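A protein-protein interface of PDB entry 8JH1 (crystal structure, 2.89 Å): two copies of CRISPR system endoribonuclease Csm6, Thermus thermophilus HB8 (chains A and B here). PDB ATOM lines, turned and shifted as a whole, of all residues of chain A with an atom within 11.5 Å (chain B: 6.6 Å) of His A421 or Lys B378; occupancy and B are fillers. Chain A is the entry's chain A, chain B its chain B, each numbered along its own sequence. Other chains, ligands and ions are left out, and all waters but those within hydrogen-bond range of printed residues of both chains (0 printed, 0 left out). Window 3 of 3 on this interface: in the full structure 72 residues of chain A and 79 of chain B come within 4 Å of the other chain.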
ATOM      1  N   VAL A 320      15.490 -28.980  13.208  1.00  0.00           N
ATOM      2  CA  VAL A 320      14.920 -28.619  11.910  1.00  0.00           C
ATOM      3  C   VAL A 320      13.450 -28.277  12.069  1.00  0.00           C
ATOM      4  O   VAL A 320      12.990 -27.196  11.670  1.00  0.00           O
ATOM      5  CB  VAL A 320      15.094 -29.760  10.902  1.00  0.00           C
ATOM      6  CG1 VAL A 320      14.545 -29.311   9.549  1.00  0.00           C
ATOM      7  CG2 VAL A 320      16.565 -30.203  10.840  1.00  0.00           C
ATOM      8  N   ALA A 323      12.750 -24.820  13.365  1.00  0.00           N
ATOM      9  CA  ALA A 323      12.811 -23.762  12.365  1.00  0.00           C
ATOM     10  C   ALA A 323      11.585 -23.763  11.460  1.00  0.00           C
ATOM     11  O   ALA A 323      11.067 -22.694  11.131  1.00  0.00           O
ATOM     12  CB  ALA A 323      14.084 -23.890  11.534  1.00  0.00           C
ATOM     13  N   LEU A 324      11.124 -24.931  11.004  1.00  0.00           N
ATOM     14  CA  LEU A 324       9.940 -24.905  10.148  1.00  0.00           C
ATOM     15  C   LEU A 324       8.773 -24.246  10.868  1.00  0.00           C
ATOM     16  O   LEU A 324       8.086 -23.383  10.307  1.00  0.00           O
ATOM     17  CB  LEU A 324       9.547 -26.304   9.678  1.00  0.00           C
ATOM     18  CG  LEU A 324      10.294 -26.912   8.498  1.00  0.00           C
ATOM     19  CD1 LEU A 324      11.788 -26.880   8.690  1.00  0.00           C
ATOM     20  CD2 LEU A 324       9.807 -28.314   8.250  1.00  0.00           C
ATOM     21  N   TYR A 327       9.376 -20.387  11.057  1.00  0.00           N
ATOM     22  CA  TYR A 327       9.132 -19.724   9.779  1.00  0.00           C
ATOM     23  C   TYR A 327       7.645 -19.622   9.499  1.00  0.00           C
ATOM     24  O   TYR A 327       7.160 -18.580   9.045  1.00  0.00           O
ATOM     25  CB  TYR A 327       9.820 -20.472   8.640  1.00  0.00           C
ATOM     26  CG  TYR A 327      11.295 -20.228   8.588  1.00  0.00           C
ATOM     27  CD1 TYR A 327      11.794 -18.940   8.460  1.00  0.00           C
ATOM     28  CD2 TYR A 327      12.190 -21.279   8.646  1.00  0.00           C
ATOM     29  CE1 TYR A 327      13.137 -18.705   8.414  1.00  0.00           C
ATOM     30  CE2 TYR A 327      13.546 -21.057   8.598  1.00  0.00           C
ATOM     31  CZ  TYR A 327      14.010 -19.766   8.480  1.00  0.00           C
ATOM     32  OH  TYR A 327      15.360 -19.538   8.430  1.00  0.00           O
ATOM     33  N   LYS A 412      16.779 -16.065   4.987  1.00  0.00           N
ATOM     34  CA  LYS A 412      17.327 -16.841   3.879  1.00  0.00           C
ATOM     35  C   LYS A 412      17.403 -18.327   4.232  1.00  0.00           C
ATOM     36  O   LYS A 412      17.364 -19.180   3.333  1.00  0.00           O
ATOM     37  CB  LYS A 412      18.717 -16.274   3.520  1.00  0.00           C
ATOM     38  CG  LYS A 412      19.720 -17.081   2.649  1.00  0.00           C
ATOM     39  CD  LYS A 412      19.152 -17.909   1.480  1.00  0.00           C
ATOM     40  CE  LYS A 412      20.225 -18.197   0.431  1.00  0.00           C
ATOM     41  NZ  LYS A 412      20.923 -19.514   0.667  1.00  0.00           N
ATOM     42  N   GLY A 413      17.465 -18.654   5.530  1.00  0.00           N
ATOM     43  CA  GLY A 413      17.536 -20.053   5.948  1.00  0.00           C
ATOM     44  C   GLY A 413      16.471 -20.966   5.351  1.00  0.00           C
ATOM     45  O   GLY A 413      16.756 -22.135   5.076  1.00  0.00           O
ATOM     46  N   ARG A 414      15.243 -20.454   5.144  1.00  0.00           N
ATOM     47  CA  ARG A 414      14.176 -21.192   4.456  1.00  0.00           C
ATOM     48  C   ARG A 414      14.664 -21.734   3.108  1.00  0.00           C
ATOM     49  O   ARG A 414      15.643 -21.251   2.529  1.00  0.00           O
ATOM     50  CB  ARG A 414      12.947 -20.299   4.254  1.00  0.00           C
ATOM     51  CG  ARG A 414      13.199 -18.986   3.477  1.00  0.00           C
ATOM     52  CD  ARG A 414      12.863 -19.031   1.969  1.00  0.00           C
ATOM     53  NE  ARG A 414      12.555 -17.684   1.484  1.00  0.00           N
ATOM     54  CZ  ARG A 414      11.348 -17.128   1.478  1.00  0.00           C
ATOM     55  NH1 ARG A 414      10.276 -17.811   1.829  1.00  0.00           N
ATOM     56  NH2 ARG A 414      11.221 -15.850   1.120  1.00  0.00           N
ATOM     57  N   ASN A 415      13.966 -22.762   2.608  1.00  0.00           N
ATOM     58  CA  ASN A 415      14.577 -23.736   1.702  1.00  0.00           C
ATOM     59  C   ASN A 415      15.801 -24.255   2.437  1.00  0.00           C
ATOM     60  O   ASN A 415      15.852 -24.120   3.660  1.00  0.00           O
ATOM     61  CB  ASN A 415      14.927 -23.139   0.342  1.00  0.00           C
ATOM     62  CG  ASN A 415      13.767 -23.212  -0.630  1.00  0.00           C
ATOM     63  OD1 ASN A 415      13.929 -23.647  -1.776  1.00  0.00           O
ATOM     64  ND2 ASN A 415      12.584 -22.785  -0.180  1.00  0.00           N
ATOM     65  N   SER A 416      16.795 -24.814   1.748  1.00  0.00           N
ATOM     66  CA  SER A 416      17.956 -25.402   2.441  1.00  0.00           C
ATOM     67  C   SER A 416      17.396 -26.398   3.458  1.00  0.00           C
ATOM     68  O   SER A 416      16.570 -27.234   3.063  1.00  0.00           O
ATOM     69  CB  SER A 416      18.814 -24.278   3.019  1.00  0.00           C
ATOM     70  OG  SER A 416      19.086 -23.292   2.041  1.00  0.00           O
ATOM     71  N   ALA A 417      17.816 -26.365   4.736  1.00  0.00           N
ATOM     72  CA  ALA A 417      16.928 -26.747   5.839  1.00  0.00           C
ATOM     73  C   ALA A 417      16.330 -28.136   5.687  1.00  0.00           C
ATOM     74  O   ALA A 417      15.253 -28.279   5.108  1.00  0.00           O
ATOM     75  CB  ALA A 417      15.809 -25.728   6.056  1.00  0.00           C
ATOM     76  N   LEU A 418      17.042 -29.158   6.141  1.00  0.00           N
ATOM     77  CA  LEU A 418      16.837 -30.557   5.791  1.00  0.00           C
ATOM     78  C   LEU A 418      15.416 -30.923   5.394  1.00  0.00           C
ATOM     79  O   LEU A 418      15.201 -31.502   4.328  1.00  0.00           O
ATOM     80  CB  LEU A 418      17.231 -31.410   6.993  1.00  0.00           C
ATOM     81  CG  LEU A 418      17.429 -32.894   6.752  1.00  0.00           C
ATOM     82  CD1 LEU A 418      18.589 -33.105   5.788  1.00  0.00           C
ATOM     83  CD2 LEU A 418      17.677 -33.572   8.072  1.00  0.00           C
ATOM     84  N   LEU A 419      14.433 -30.568   6.197  1.00  0.00           N
ATOM     85  CA  LEU A 419      13.079 -30.983   5.860  1.00  0.00           C
ATOM     86  C   LEU A 419      12.417 -30.136   4.763  1.00  0.00           C
ATOM     87  O   LEU A 419      11.219 -30.321   4.526  1.00  0.00           O
ATOM     88  CB  LEU A 419      12.211 -30.985   7.115  1.00  0.00           C
ATOM     89  CG  LEU A 419      12.662 -32.113   8.028  1.00  0.00           C
ATOM     90  CD1 LEU A 419      12.142 -31.900   9.422  1.00  0.00           C
ATOM     91  CD2 LEU A 419      12.287 -33.480   7.472  1.00  0.00           C
ATOM     92  N   VAL A 420      13.133 -29.241   4.072  1.00  0.00           N
ATOM     93  CA  VAL A 420      12.479 -28.504   2.994  1.00  0.00           C
ATOM     94  C   VAL A 420      13.045 -28.890   1.628  1.00  0.00           C
ATOM     95  O   VAL A 420      12.440 -29.691   0.903  1.00  0.00           O
ATOM     96  CB  VAL A 420      12.614 -26.976   3.204  1.00  0.00           C
ATOM     97  CG1 VAL A 420      11.565 -26.232   2.395  1.00  0.00           C
ATOM     98  CG2 VAL A 420      12.515 -26.601   4.674  1.00  0.00           C
ATOM     99  N   HIS A 421      14.250 -28.397   1.304  1.00  0.00           N
ATOM    100  CA  HIS A 421      14.808 -28.553  -0.038  1.00  0.00           C
ATOM    101  C   HIS A 421      16.315 -28.790  -0.047  1.00  0.00           C
ATOM    102  O   HIS A 421      16.900 -28.879  -1.132  1.00  0.00           O
ATOM    103  CB  HIS A 421      14.483 -27.312  -0.897  1.00  0.00           C
ATOM    104  CG  HIS A 421      13.052 -27.227  -1.341  1.00  0.00           C
ATOM    105  ND1 HIS A 421      12.356 -28.306  -1.845  1.00  0.00           N
ATOM    106  CD2 HIS A 421      12.192 -26.181  -1.373  1.00  0.00           C
ATOM    107  CE1 HIS A 421      11.129 -27.932  -2.163  1.00  0.00           C
ATOM    108  NE2 HIS A 421      11.002 -26.647  -1.886  1.00  0.00           N
ATOM    109  N   GLY A 422      16.952 -28.896   1.116  1.00  0.00           N
ATOM    110  CA  GLY A 422      18.391 -28.970   1.245  1.00  0.00           C
ATOM    111  C   GLY A 422      18.806 -29.850   2.404  1.00  0.00           C
ATOM    112  O   GLY A 422      18.089 -30.788   2.743  1.00  0.00           O
ATOM    113  N   PHE A 423      19.991 -29.617   2.972  1.00  0.00           N
ATOM    114  CA  PHE A 423      20.513 -30.418   4.081  1.00  0.00           C
ATOM    115  C   PHE A 423      21.102 -29.471   5.125  1.00  0.00           C
ATOM    116  O   PHE A 423      22.318 -29.305   5.205  1.00  0.00           O
ATOM    117  CB  PHE A 423      21.557 -31.410   3.560  1.00  0.00           C
ATOM    118  CG  PHE A 423      21.224 -31.979   2.209  1.00  0.00           C
ATOM    119  CD1 PHE A 423      21.446 -31.239   1.059  1.00  0.00           C
ATOM    120  CD2 PHE A 423      20.691 -33.254   2.087  1.00  0.00           C
ATOM    121  CE1 PHE A 423      21.118 -31.743  -0.176  1.00  0.00           C
ATOM    122  CE2 PHE A 423      20.369 -33.772   0.845  1.00  0.00           C
ATOM    123  CZ  PHE A 423      20.588 -33.014  -0.288  1.00  0.00           C
ATOM    124  N   ASP A 424      20.256 -28.874   5.961  1.00  0.00           N
ATOM    125  CA  ASP A 424      20.743 -27.950   6.986  1.00  0.00           C
ATOM    126  C   ASP A 424      19.923 -28.086   8.251  1.00  0.00           C
ATOM    127  O   ASP A 424      18.696 -27.960   8.214  1.00  0.00           O
ATOM    128  CB  ASP A 424      20.677 -26.482   6.546  1.00  0.00           C
ATOM    129  CG  ASP A 424      20.933 -26.302   5.080  1.00  0.00           C
ATOM    130  OD1 ASP A 424      20.063 -26.734   4.295  1.00  0.00           O
ATOM    131  OD2 ASP A 424      21.984 -25.715   4.721  1.00  0.00           O
ATOM    132  N   VAL A 425      20.600 -28.296   9.370  1.00  0.00           N
ATOM    133  CA  VAL A 425      19.964 -28.034  10.653  1.00  0.00           C
ATOM    134  C   VAL A 425      20.238 -26.566  10.956  1.00  0.00           C
ATOM    135  O   VAL A 425      21.346 -26.232  11.398  1.00  0.00           O
ATOM    136  CB  VAL A 425      20.493 -28.961  11.752  1.00  0.00           C
ATOM    137  CG1 VAL A 425      19.726 -28.712  13.042  1.00  0.00           C
ATOM    138  CG2 VAL A 425      20.399 -30.424  11.302  1.00  0.00           C
ATOM    139  N   PRO A 426      19.287 -25.661  10.717  1.00  0.00           N
ATOM    140  CA  PRO A 426      19.599 -24.228  10.807  1.00  0.00           C
ATOM    141  C   PRO A 426      19.966 -23.845  12.230  1.00  0.00           C
ATOM    142  O   PRO A 426      19.531 -24.479  13.197  1.00  0.00           O
ATOM    143  CB  PRO A 426      18.308 -23.537  10.342  1.00  0.00           C
ATOM    144  CG  PRO A 426      17.248 -24.576  10.344  1.00  0.00           C
ATOM    145  CD  PRO A 426      17.839 -25.922  10.593  1.00  0.00           C
ATOM    146  N   ARG B 328       9.951 -34.736   1.623  1.00  0.00           N
ATOM    147  CA  ARG B 328      11.408 -34.617   1.620  1.00  0.00           C
ATOM    148  C   ARG B 328      12.054 -35.907   1.132  1.00  0.00           C
ATOM    149  O   ARG B 328      13.049 -35.871   0.398  1.00  0.00           O
ATOM    150  CB  ARG B 328      11.923 -34.237   3.012  1.00  0.00           C
ATOM    151  CG  ARG B 328      13.329 -33.676   3.011  1.00  0.00           C
ATOM    152  CD  ARG B 328      13.614 -32.906   1.728  1.00  0.00           C
ATOM    153  NE  ARG B 328      14.936 -32.294   1.753  1.00  0.00           N
ATOM    154  CZ  ARG B 328      15.888 -32.524   0.855  1.00  0.00           C
ATOM    155  NH1 ARG B 328      15.676 -33.301  -0.197  1.00  0.00           N
ATOM    156  NH2 ARG B 328      17.086 -31.972   1.022  1.00  0.00           N
ATOM    157  N   GLU B 331      11.773 -36.076  -2.632  1.00  0.00           N
ATOM    158  CA  GLU B 331      12.732 -35.155  -3.233  1.00  0.00           C
ATOM    159  C   GLU B 331      14.132 -35.735  -3.189  1.00  0.00           C
ATOM    160  O   GLU B 331      14.876 -35.643  -4.167  1.00  0.00           O
ATOM    161  CB  GLU B 331      12.707 -33.780  -2.550  1.00  0.00           C
ATOM    162  CG  GLU B 331      13.262 -32.663  -3.464  1.00  0.00           C
ATOM    163  CD  GLU B 331      13.341 -31.281  -2.812  1.00  0.00           C
ATOM    164  OE1 GLU B 331      13.717 -31.180  -1.622  1.00  0.00           O
ATOM    165  OE2 GLU B 331      13.075 -30.282  -3.513  1.00  0.00           O
ATOM    166  N   GLN B 335      16.162 -36.657  -6.502  1.00  0.00           N
ATOM    167  CA  GLN B 335      17.408 -35.949  -6.768  1.00  0.00           C
ATOM    168  C   GLN B 335      18.567 -36.923  -6.927  1.00  0.00           C
ATOM    169  O   GLN B 335      19.479 -36.684  -7.729  1.00  0.00           O
ATOM    170  CB  GLN B 335      17.686 -34.934  -5.654  1.00  0.00           C
ATOM    171  CG  GLN B 335      16.864 -33.666  -5.749  1.00  0.00           C
ATOM    172  CD  GLN B 335      16.919 -32.817  -4.487  1.00  0.00           C
ATOM    173  OE1 GLN B 335      17.235 -33.309  -3.399  1.00  0.00           O
ATOM    174  NE2 GLN B 335      16.616 -31.523  -4.631  1.00  0.00           N
ATOM    175  N   ALA B 345      19.368 -31.188  -9.649  1.00  0.00           N
ATOM    176  CA  ALA B 345      18.103 -30.450  -9.708  1.00  0.00           C
ATOM    177  C   ALA B 345      18.126 -29.285  -8.737  1.00  0.00           C
ATOM    178  O   ALA B 345      17.905 -29.470  -7.534  1.00  0.00           O
ATOM    179  CB  ALA B 345      16.926 -31.358  -9.382  1.00  0.00           C
ATOM    180  N   GLU B 346      18.301 -28.081  -9.280  1.00  0.00           N
ATOM    181  CA  GLU B 346      18.612 -26.853  -8.555  1.00  0.00           C
ATOM    182  C   GLU B 346      19.280 -25.958  -9.586  1.00  0.00           C
ATOM    183  O   GLU B 346      19.112 -24.736  -9.584  1.00  0.00           O
ATOM    184  CB  GLU B 346      19.534 -27.085  -7.342  1.00  0.00           C
ATOM    185  CG  GLU B 346      21.027 -26.952  -7.656  1.00  0.00           C
ATOM    186  CD  GLU B 346      21.912 -27.901  -6.864  1.00  0.00           C
ATOM    187  OE1 GLU B 346      21.694 -29.125  -6.987  1.00  0.00           O
ATOM    188  OE2 GLU B 346      22.843 -27.432  -6.166  1.00  0.00           O
ATOM    189  N   ALA B 347      20.042 -26.585 -10.474  1.00  0.00           N
ATOM    190  CA  ALA B 347      20.672 -25.962 -11.621  1.00  0.00           C
ATOM    191  C   ALA B 347      20.884 -27.024 -12.695  1.00  0.00           C
ATOM    192  O   ALA B 347      22.028 -27.287 -13.088  1.00  0.00           O
ATOM    193  CB  ALA B 347      21.996 -25.310 -11.224  1.00  0.00           C
ATOM    194  N   PRO B 348      19.828 -27.671 -13.182  1.00  0.00           N
ATOM    195  CA  PRO B 348      20.009 -28.604 -14.292  1.00  0.00           C
ATOM    196  C   PRO B 348      20.250 -27.824 -15.571  1.00  0.00           C
ATOM    197  O   PRO B 348      19.721 -26.725 -15.761  1.00  0.00           O
ATOM    198  CB  PRO B 348      18.678 -29.356 -14.341  1.00  0.00           C
ATOM    199  CG  PRO B 348      17.685 -28.336 -13.903  1.00  0.00           C
ATOM    200  CD  PRO B 348      18.395 -27.411 -12.933  1.00  0.00           C
ATOM    201  N   LEU B 375       8.829 -22.771 -16.664  1.00  0.00           N
ATOM    202  CA  LEU B 375       9.746 -23.658 -15.960  1.00  0.00           C
ATOM    203  C   LEU B 375      10.476 -22.876 -14.852  1.00  0.00           C
ATOM    204  O   LEU B 375      11.066 -21.839 -15.148  1.00  0.00           O
ATOM    205  CB  LEU B 375      10.750 -24.266 -16.924  1.00  0.00           C
ATOM    206  CG  LEU B 375      10.154 -25.434 -17.695  1.00  0.00           C
ATOM    207  CD1 LEU B 375      11.242 -26.386 -18.102  1.00  0.00           C
ATOM    208  CD2 LEU B 375       9.101 -26.143 -16.845  1.00  0.00           C
ATOM    209  N   PRO B 376      10.415 -23.333 -13.602  1.00  0.00           N
ATOM    210  CA  PRO B 376      11.227 -22.673 -12.563  1.00  0.00           C
ATOM    211  C   PRO B 376      12.694 -23.003 -12.766  1.00  0.00           C
ATOM    212  O   PRO B 376      13.059 -23.936 -13.485  1.00  0.00           O
ATOM    213  CB  PRO B 376      10.693 -23.263 -11.249  1.00  0.00           C
ATOM    214  CG  PRO B 376       9.544 -24.190 -11.630  1.00  0.00           C
ATOM    215  CD  PRO B 376       9.718 -24.515 -13.085  1.00  0.00           C
ATOM    216  N   ALA B 377      13.547 -22.189 -12.142  1.00  0.00           N
ATOM    217  CA  ALA B 377      14.986 -22.352 -12.324  1.00  0.00           C
ATOM    218  C   ALA B 377      15.495 -23.621 -11.637  1.00  0.00           C
ATOM    219  O   ALA B 377      16.283 -24.377 -12.220  1.00  0.00           O
ATOM    220  CB  ALA B 377      15.722 -21.110 -11.820  1.00  0.00           C
ATOM    221  N   LYS B 378      15.079 -23.856 -10.388  1.00  0.00           N
ATOM    222  CA  LYS B 378      15.262 -25.159  -9.757  1.00  0.00           C
ATOM    223  C   LYS B 378      14.094 -26.062 -10.136  1.00  0.00           C
ATOM    224  O   LYS B 378      12.930 -25.641 -10.118  1.00  0.00           O
ATOM    225  CB  LYS B 378      15.354 -25.046  -8.223  1.00  0.00           C
ATOM    226  CG  LYS B 378      14.991 -26.359  -7.461  1.00  0.00           C
ATOM    227  CD  LYS B 378      15.094 -26.268  -5.926  1.00  0.00           C
ATOM    228  CE  LYS B 378      13.933 -27.016  -5.231  1.00  0.00           C
ATOM    229  NZ  LYS B 378      13.836 -28.469  -5.575  1.00  0.00           N
ATOM    230  N   LEU B 379      14.406 -27.304 -10.490  1.00  0.00           N
ATOM    231  CA  LEU B 379      13.364 -28.308 -10.642  1.00  0.00           C
ATOM    232  C   LEU B 379      12.809 -28.672  -9.269  1.00  0.00           C
ATOM    233  O   LEU B 379      13.496 -29.298  -8.453  1.00  0.00           O
ATOM    234  CB  LEU B 379      13.922 -29.534 -11.348  1.00  0.00           C
ATOM    235  CG  LEU B 379      14.474 -29.236 -12.731  1.00  0.00           C
ATOM    236  CD1 LEU B 379      14.649 -30.535 -13.490  1.00  0.00           C
ATOM    237  CD2 LEU B 379      13.549 -28.286 -13.478  1.00  0.00           C
ATOM    238  N   GLY B 380      11.574 -28.264  -9.003  1.00  0.00           N
ATOM    239  CA  GLY B 380      10.849 -28.771  -7.869  1.00  0.00           C
ATOM    240  C   GLY B 380      10.365 -30.176  -8.145  1.00  0.00           C
ATOM    241  O   GLY B 380      10.684 -30.796  -9.160  1.00  0.00           O
ATOM    242  N   LEU B 381       9.551 -30.673  -7.221  1.00  0.00           N
ATOM    243  CA  LEU B 381       9.310 -32.106  -7.138  1.00  0.00           C
ATOM    244  C   LEU B 381       8.593 -32.642  -8.373  1.00  0.00           C
ATOM    245  O   LEU B 381       8.981 -33.668  -8.939  1.00  0.00           O
ATOM    246  CB  LEU B 381       8.522 -32.396  -5.876  1.00  0.00           C
ATOM    247  CG  LEU B 381       8.853 -33.765  -5.330  1.00  0.00           C
ATOM    248  CD1 LEU B 381      10.296 -33.686  -5.001  1.00  0.00           C
ATOM    249  CD2 LEU B 381       8.030 -34.081  -4.099  1.00  0.00           C
ATOM    250  N   ASP B 383       8.379 -31.108 -11.348  1.00  0.00           N
ATOM    251  CA  ASP B 383       9.263 -30.887 -12.484  1.00  0.00           C
ATOM    252  C   ASP B 383      10.305 -31.998 -12.563  1.00  0.00           C
ATOM    253  O   ASP B 383      10.546 -32.562 -13.638  1.00  0.00           O
ATOM    254  CB  ASP B 383       9.929 -29.509 -12.364  1.00  0.00           C
ATOM    255  CG  ASP B 383       8.939 -28.393 -11.991  1.00  0.00           C
ATOM    256  OD1 ASP B 383       8.174 -27.931 -12.877  1.00  0.00           O
ATOM    257  OD2 ASP B 383       8.932 -27.965 -10.810  1.00  0.00           O
ATOM    258  N   LEU B 384      10.890 -32.358 -11.414  1.00  0.00           N
ATOM    259  CA  LEU B 384      11.864 -33.447 -11.341  1.00  0.00           C
ATOM    260  C   LEU B 384      11.257 -34.780 -11.769  1.00  0.00           C
ATOM    261  O   LEU B 384      11.882 -35.542 -12.514  1.00  0.00           O
ATOM    262  CB  LEU B 384      12.402 -33.544  -9.911  1.00  0.00           C
ATOM    263  CG  LEU B 384      13.846 -33.966  -9.688  1.00  0.00           C
ATOM    264  CD1 LEU B 384      14.683 -33.480 -10.855  1.00  0.00           C
ATOM    265  CD2 LEU B 384      14.321 -33.402  -8.356  1.00  0.00           C
ATOM    266  N   ARG B 414       2.536 -29.534  -2.118  1.00  0.00           N
ATOM    267  CA  ARG B 414       3.805 -29.122  -1.520  1.00  0.00           C
ATOM    268  C   ARG B 414       3.972 -27.604  -1.620  1.00  0.00           C
ATOM    269  O   ARG B 414       4.231 -26.936  -0.610  1.00  0.00           O
ATOM    270  CB  ARG B 414       4.981 -29.864  -2.183  1.00  0.00           C
ATOM    271  CG  ARG B 414       6.371 -29.657  -1.528  1.00  0.00           C
ATOM    272  CD  ARG B 414       7.336 -28.887  -2.446  1.00  0.00           C
ATOM    273  NE  ARG B 414       7.123 -29.201  -3.858  1.00  0.00           N
ATOM    274  CZ  ARG B 414       7.790 -28.656  -4.870  1.00  0.00           C
ATOM    275  NH1 ARG B 414       8.767 -27.784  -4.669  1.00  0.00           N
ATOM    276  NH2 ARG B 414       7.456 -28.983  -6.117  1.00  0.00           N
ATOM    277  N   VAL B 420       4.383 -25.421   4.954  1.00  0.00           N
ATOM    278  CA  VAL B 420       5.155 -24.848   3.861  1.00  0.00           C
ATOM    279  C   VAL B 420       4.573 -23.463   3.642  1.00  0.00           C
ATOM    280  O   VAL B 420       3.597 -23.092   4.301  1.00  0.00           O
ATOM    281  CB  VAL B 420       5.094 -25.722   2.594  1.00  0.00           C
ATOM    282  CG1 VAL B 420       6.242 -25.394   1.661  1.00  0.00           C
ATOM    283  CG2 VAL B 420       5.130 -27.195   2.967  1.00  0.00           C
ATOM    284  N   HIS B 421       5.167 -22.675   2.746  1.00  0.00           N
ATOM    285  CA  HIS B 421       4.657 -21.331   2.515  1.00  0.00           C
ATOM    286  C   HIS B 421       3.287 -21.492   1.865  1.00  0.00           C
ATOM    287  O   HIS B 421       3.179 -21.615   0.638  1.00  0.00           O
ATOM    288  CB  HIS B 421       5.616 -20.514   1.630  1.00  0.00           C
ATOM    289  CG  HIS B 421       7.073 -20.660   1.987  1.00  0.00           C
ATOM    290  ND1 HIS B 421       7.941 -21.469   1.277  1.00  0.00           N
ATOM    291  CD2 HIS B 421       7.827 -20.058   2.940  1.00  0.00           C
ATOM    292  CE1 HIS B 421       9.155 -21.382   1.793  1.00  0.00           C
ATOM    293  NE2 HIS B 421       9.116 -20.531   2.802  1.00  0.00           N
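Arg A414 touches His B421, and with the chains exchanged His A421 touches Arg B414. Positions printed for both chains: 414, 420 and 421.
The backbone carbonyl oxygen (O) of Ser A416 lies within hydrogen-bond range of the backbone NH (N) of His A421 (3.1 Å). The backbone carbonyl oxygen (O) of Glu B331 sits close to the side-chain amide oxygen (OE1) of Gln B335 (3.4 Å). The side-chain amino group (NZ) of Lys B378 is in salt-bridge range of the side-chain carboxylate (OE2) of Glu B331, at 2.8 Å. The side-chain hydroxyl (OH) of Tyr A327 is in hydrogen-bond range of the backbone NH (N) of Arg A414. N of Gly A422 lies within hydrogen-bond range of O of Ser A416. The guanidinium group (NH1) of Arg B328 lies within salt-bridge range of the side-chain carboxylate (OE1) of Glu B331 (3.2 Å).
Leu A419 touches Arg B328. Val A420 touches Arg B328. Arg B328 touches His A421. His A421 touches Lys B378. Arg B414 touches His A421 (NH1 to CE1, 3.4 Å). Phe A423 touches Arg B328.
The guanidinium group (NH1) of Arg A414 lies within hydrogen-bond range of a ring nitrogen (NE2) of His B421, 3.1 Å away. OE2 of Glu B331 is in hydrogen-bond range of ND1 of His A421 (2.7 Å). O of Val A420 lies close to OE1 of Glu B331. The guanidinium group of Arg B328 lies within hydrogen-bond range of the backbone carbonyl oxygen of Leu A418 (2.7 Å). The guanidinium group (NH2) of Arg B328 sits close to the backbone carbonyl oxygen (O) of Gly A422, at 2.3 Å.
Of the 19 printed residues of chain A, 7 touch a printed residue of chain B. Printed residues of chain A that touch a printed residue of chain B: Arg A414, Leu A418, Leu A419, Val A420, His A421, Gly A422 and Phe A423. Hydrophobic or aromatic side chains of chain A within 4 Å of the printed part of chain B: His A421 and Phe A423. Of the 19 printed residues of chain B, 5 touch a printed residue of chain A. Printed residues of chain B that touch a printed residue of chain A: Arg B328, Glu B331, Lys B378, Arg B414 and His B421. Hydrophobic or aromatic side chains of chain B within 4 Å of the printed part of chain A: His B421. Among the printed residues, no Asp or Glu carboxylate lies within 4 Å of a Lys or Arg side-chain nitrogen of the other chain.
Of the printed residues of chain B, Arg A414 touches His B421. Of the printed residues of chain B, Leu A419 touches Arg B328 (3.9 Å). Printed residues of chain B within 4 Å of His A421: Arg B328 (3.4 Å), Glu B331 (2.7 Å), Lys B378 (3.95 Å) and Arg B414 (3.4 Å). Of the printed residues of chain B, Phe A423 touches Arg B328 (3.7 Å). Printed residues of chain A within 4 Å of Arg B328: Leu A418 (2.7 Å), Leu A419 (3.9 Å), Val A420 (3.5 Å), His A421 (3.4 Å), Gly A422 (2.3 Å) and Phe A423 (3.7 Å). No residue of chain A comes within 4 Å of Ala B377. No residue of chain A comes within 4 Å of Leu B379. No residue of chain A comes within 4 Å of Gly B380. Of the printed residues of chain A, His B421 touches Arg A414. The nearest printed residue of chain B that does not touch Leu A418 is Glu B331 (6.1 Å).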
